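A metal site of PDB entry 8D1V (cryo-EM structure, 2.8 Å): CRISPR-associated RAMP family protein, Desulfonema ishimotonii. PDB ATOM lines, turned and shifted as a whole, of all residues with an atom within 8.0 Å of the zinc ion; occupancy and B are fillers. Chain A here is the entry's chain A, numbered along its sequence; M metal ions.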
ATOM      1  N   ARG A 452      24.401  16.465  -6.682  1.00  0.00           N
ATOM      2  CA  ARG A 452      23.301  15.557  -6.962  1.00  0.00           C
ATOM      3  C   ARG A 452      21.999  16.060  -6.366  1.00  0.00           C
ATOM      4  O   ARG A 452      20.931  15.974  -6.989  1.00  0.00           O
ATOM      5  CB  ARG A 452      23.624  14.154  -6.447  1.00  0.00           C
ATOM      6  CG  ARG A 452      22.428  13.228  -6.412  1.00  0.00           C
ATOM      7  CD  ARG A 452      22.804  11.853  -5.911  1.00  0.00           C
ATOM      8  NE  ARG A 452      23.955  11.314  -6.629  1.00  0.00           N
ATOM      9  CZ  ARG A 452      23.918  10.840  -7.865  1.00  0.00           C
ATOM     10  NH1 ARG A 452      22.804  10.848  -8.575  1.00  0.00           N
ATOM     11  NH2 ARG A 452      25.027  10.355  -8.407  1.00  0.00           N
ATOM     12  N   GLN A 456      18.684  17.523  -8.635  1.00  0.00           N
ATOM     13  CA  GLN A 456      17.317  17.045  -8.484  1.00  0.00           C
ATOM     14  C   GLN A 456      16.343  18.192  -8.248  1.00  0.00           C
ATOM     15  O   GLN A 456      15.213  18.163  -8.751  1.00  0.00           O
ATOM     16  CB  GLN A 456      17.245  16.034  -7.337  1.00  0.00           C
ATOM     17  CG  GLN A 456      17.717  14.657  -7.726  1.00  0.00           C
ATOM     18  CD  GLN A 456      18.197  13.857  -6.539  1.00  0.00           C
ATOM     19  OE1 GLN A 456      17.539  12.927  -6.095  1.00  0.00           O
ATOM     20  NE2 GLN A 456      19.366  14.215  -6.021  1.00  0.00           N
ATOM     21  N   SER A 461      12.511  16.509 -10.030  1.00  0.00           N
ATOM     22  CA  SER A 461      12.310  15.082 -10.003  1.00  0.00           C
ATOM     23  C   SER A 461      13.388  14.432  -9.153  1.00  0.00           C
ATOM     24  O   SER A 461      14.576  14.529  -9.496  1.00  0.00           O
ATOM     25  CB  SER A 461      12.356  14.497 -11.424  1.00  0.00           C
ATOM     26  OG  SER A 461      11.368  15.086 -12.265  1.00  0.00           O
ATOM     27  N   PRO A 462      13.040  13.792  -8.046  1.00  0.00           N
ATOM     28  CA  PRO A 462      14.034  13.031  -7.295  1.00  0.00           C
ATOM     29  C   PRO A 462      14.472  11.799  -8.069  1.00  0.00           C
ATOM     30  O   PRO A 462      13.838  11.368  -9.030  1.00  0.00           O
ATOM     31  CB  PRO A 462      13.308  12.654  -6.001  1.00  0.00           C
ATOM     32  CG  PRO A 462      12.075  13.521  -5.964  1.00  0.00           C
ATOM     33  CD  PRO A 462      11.727  13.791  -7.392  1.00  0.00           C
ATOM     34  N   CYS A 463      15.605  11.238  -7.648  1.00  0.00           N
ATOM     35  CA  CYS A 463      16.125   9.999  -8.190  1.00  0.00           C
ATOM     36  C   CYS A 463      15.873   8.891  -7.176  1.00  0.00           C
ATOM     37  O   CYS A 463      16.387   8.929  -6.053  1.00  0.00           O
ATOM     38  CB  CYS A 463      17.612  10.113  -8.507  1.00  0.00           C
ATOM     39  SG  CYS A 463      18.337   8.541  -9.011  1.00  0.00           S
ATOM     40  N   ASN A 464      15.066   7.911  -7.563  1.00  0.00           N
ATOM     41  CA  ASN A 464      14.665   6.820  -6.676  1.00  0.00           C
ATOM     42  C   ASN A 464      15.438   5.535  -6.933  1.00  0.00           C
ATOM     43  O   ASN A 464      15.066   4.487  -6.387  1.00  0.00           O
ATOM     44  CB  ASN A 464      13.161   6.584  -6.787  1.00  0.00           C
ATOM     45  CG  ASN A 464      12.713   6.132  -8.173  1.00  0.00           C
ATOM     46  OD1 ASN A 464      13.527   5.870  -9.051  1.00  0.00           O
ATOM     47  ND2 ASN A 464      11.405   6.039  -8.356  1.00  0.00           N
ATOM     48  N   ALA A 465      16.493   5.575  -7.737  1.00  0.00           N
ATOM     49  CA  ALA A 465      17.272   4.381  -8.020  1.00  0.00           C
ATOM     50  C   ALA A 465      17.985   3.886  -6.769  1.00  0.00           C
ATOM     51  O   ALA A 465      18.471   4.679  -5.944  1.00  0.00           O
ATOM     52  CB  ALA A 465      18.298   4.657  -9.121  1.00  0.00           C
ATOM     53  N   GLU A 466      18.048   2.572  -6.622  1.00  0.00           N
ATOM     54  CA  GLU A 466      18.723   1.953  -5.497  1.00  0.00           C
ATOM     55  C   GLU A 466      20.150   1.573  -5.879  1.00  0.00           C
ATOM     56  O   GLU A 466      20.547   1.609  -7.042  1.00  0.00           O
ATOM     57  CB  GLU A 466      17.932   0.742  -4.997  1.00  0.00           C
ATOM     58  CG  GLU A 466      17.888  -0.424  -5.976  1.00  0.00           C
ATOM     59  CD  GLU A 466      16.666  -0.380  -6.875  1.00  0.00           C
ATOM     60  OE1 GLU A 466      15.862   0.553  -6.743  1.00  0.00           O
ATOM     61  OE2 GLU A 466      16.519  -1.286  -7.724  1.00  0.00           O
ATOM     62  N   PRO A 471      23.301   1.177 -14.339  1.00  0.00           N
ATOM     63  CA  PRO A 471      23.263   2.591 -13.937  1.00  0.00           C
ATOM     64  C   PRO A 471      21.914   3.240 -14.224  1.00  0.00           C
ATOM     65  O   PRO A 471      21.305   3.010 -15.271  1.00  0.00           O
ATOM     66  CB  PRO A 471      24.377   3.236 -14.781  1.00  0.00           C
ATOM     67  CG  PRO A 471      25.277   2.114 -15.118  1.00  0.00           C
ATOM     68  CD  PRO A 471      24.432   0.892 -15.231  1.00  0.00           C
ATOM     69  N   CYS A 472      21.465   4.062 -13.282  1.00  0.00           N
ATOM     70  CA  CYS A 472      20.229   4.801 -13.460  1.00  0.00           C
ATOM     71  C   CYS A 472      20.346   5.760 -14.634  1.00  0.00           C
ATOM     72  O   CYS A 472      21.372   6.415 -14.806  1.00  0.00           O
ATOM     73  CB  CYS A 472      19.883   5.566 -12.178  1.00  0.00           C
ATOM     74  SG  CYS A 472      18.223   6.288 -12.141  1.00  0.00           S
ATOM     75  N   MET A 473      19.300   5.829 -15.442  1.00  0.00           N
ATOM     76  CA  MET A 473      19.314   6.622 -16.671  1.00  0.00           C
ATOM     77  C   MET A 473      18.484   7.890 -16.555  1.00  0.00           C
ATOM     78  O   MET A 473      18.094   8.480 -17.564  1.00  0.00           O
ATOM     79  CB  MET A 473      18.839   5.770 -17.848  1.00  0.00           C
ATOM     80  CG  MET A 473      19.638   4.508 -18.072  1.00  0.00           C
ATOM     81  SD  MET A 473      21.374   4.802 -18.474  1.00  0.00           S
ATOM     82  CE  MET A 473      21.206   6.037 -19.757  1.00  0.00           C
ATOM     83  N   CYS A 474      18.210   8.344 -15.337  1.00  0.00           N
ATOM     84  CA  CYS A 474      17.496   9.594 -15.133  1.00  0.00           C
ATOM     85  C   CYS A 474      18.416  10.759 -15.443  1.00  0.00           C
ATOM     86  O   CYS A 474      19.632  10.589 -15.603  1.00  0.00           O
ATOM     87  CB  CYS A 474      16.960   9.707 -13.699  1.00  0.00           C
ATOM     88  SG  CYS A 474      18.163  10.168 -12.451  1.00  0.00           S
ATOM     89  N   LYS A 475      17.830  11.947 -15.560  1.00  0.00           N
ATOM     90  CA  LYS A 475      18.587  13.114 -15.983  1.00  0.00           C
ATOM     91  C   LYS A 475      19.690  13.451 -14.978  1.00  0.00           C
ATOM     92  O   LYS A 475      20.765  13.919 -15.373  1.00  0.00           O
ATOM     93  CB  LYS A 475      17.659  14.308 -16.180  1.00  0.00           C
ATOM     94  CG  LYS A 475      16.569  14.081 -17.205  1.00  0.00           C
ATOM     95  CD  LYS A 475      15.436  15.064 -17.044  1.00  0.00           C
ATOM     96  CE  LYS A 475      14.714  14.864 -15.710  1.00  0.00           C
ATOM     97  NZ  LYS A 475      13.581  15.805 -15.550  1.00  0.00           N
ATOM     98  N   THR A 476      19.422  13.252 -13.690  1.00  0.00           N
ATOM     99  CA  THR A 476      20.411  13.569 -12.668  1.00  0.00           C
ATOM    100  C   THR A 476      21.573  12.595 -12.705  1.00  0.00           C
ATOM    101  O   THR A 476      22.739  13.007 -12.689  1.00  0.00           O
ATOM    102  CB  THR A 476      19.752  13.576 -11.286  1.00  0.00           C
ATOM    103  OG1 THR A 476      18.864  14.692 -11.191  1.00  0.00           O
ATOM    104  CG2 THR A 476      20.798  13.667 -10.190  1.00  0.00           C
ATOM    105  N   CYS A 477      21.289  11.293 -12.774  1.00  0.00           N
ATOM    106  CA  CYS A 477      22.361  10.297 -12.823  1.00  0.00           C
ATOM    107  C   CYS A 477      23.202  10.431 -14.081  1.00  0.00           C
ATOM    108  O   CYS A 477      24.410  10.212 -14.024  1.00  0.00           O
ATOM    109  CB  CYS A 477      21.796   8.889 -12.740  1.00  0.00           C
ATOM    110  SG  CYS A 477      21.234   8.407 -11.109  1.00  0.00           S
ATOM    111  N   ARG A 478      22.590  10.754 -15.215  1.00  0.00           N
ATOM    112  CA  ARG A 478      23.346  10.899 -16.453  1.00  0.00           C
ATOM    113  C   ARG A 478      24.356  12.030 -16.357  1.00  0.00           C
ATOM    114  O   ARG A 478      25.492  11.915 -16.810  1.00  0.00           O
ATOM    115  CB  ARG A 478      22.394  11.113 -17.624  1.00  0.00           C
ATOM    116  CG  ARG A 478      21.738   9.838 -18.120  1.00  0.00           C
ATOM    117  CD  ARG A 478      21.049  10.047 -19.457  1.00  0.00           C
ATOM    118  NE  ARG A 478      19.596  10.082 -19.335  1.00  0.00           N
ATOM    119  CZ  ARG A 478      18.860  11.172 -19.464  1.00  0.00           C
ATOM    120  NH1 ARG A 478      19.406  12.350 -19.731  1.00  0.00           N
ATOM    121  NH2 ARG A 478      17.537  11.086 -19.331  1.00  0.00           N
ATOM    122  N   ARG A 481      27.316  11.104 -13.914  1.00  0.00           N
ATOM    123  CA  ARG A 481      28.300  10.136 -14.382  1.00  0.00           C
ATOM    124  C   ARG A 481      29.378  10.765 -15.248  1.00  0.00           C
ATOM    125  O   ARG A 481      30.390  10.110 -15.528  1.00  0.00           O
ATOM    126  CB  ARG A 481      27.602   9.018 -15.157  1.00  0.00           C
ATOM    127  CG  ARG A 481      27.016   7.958 -14.262  1.00  0.00           C
ATOM    128  CD  ARG A 481      26.742   6.691 -15.025  1.00  0.00           C
ATOM    129  NE  ARG A 481      25.853   6.936 -16.146  1.00  0.00           N
ATOM    130  CZ  ARG A 481      24.532   6.867 -16.082  1.00  0.00           C
ATOM    131  NH1 ARG A 481      23.917   6.532 -14.957  1.00  0.00           N
ATOM    132  NH2 ARG A 481      23.809   7.131 -17.168  1.00  0.00           N
HETATM  133 ZN    ZN M   1      18.922   8.327 -11.244  1.00  0.00          ZN
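SG of Cys 463 sits close to N of Ala 465 (3.7 Å).
N of Cys 463 lies within hydrogen-bond range of OE1 of Gln 456 (3.0 Å).
SG of Cys 474 lies close to N of Thr 476, at 3.6 Å.
The backbone carbonyl oxygen of Cys 472 is in hydrogen-bond range of the guanidinium group of Arg 481, at 2.6 Å.
Within 4 Å of the zinc ion: Cys 463, Cys 472, Cys 474 and Cys 477.
The zinc ion is bound by the side-chain sulfur (SG) of Cys 477 (2.3 Å), the side-chain sulfur (SG) of Cys 463 (2.3 Å), the side-chain sulfur (SG) of Cys 474 (2.3 Å) and the side-chain sulfur (SG) of Cys 472 (2.3 Å).
The zinc ion has four donor atoms within binding distance.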
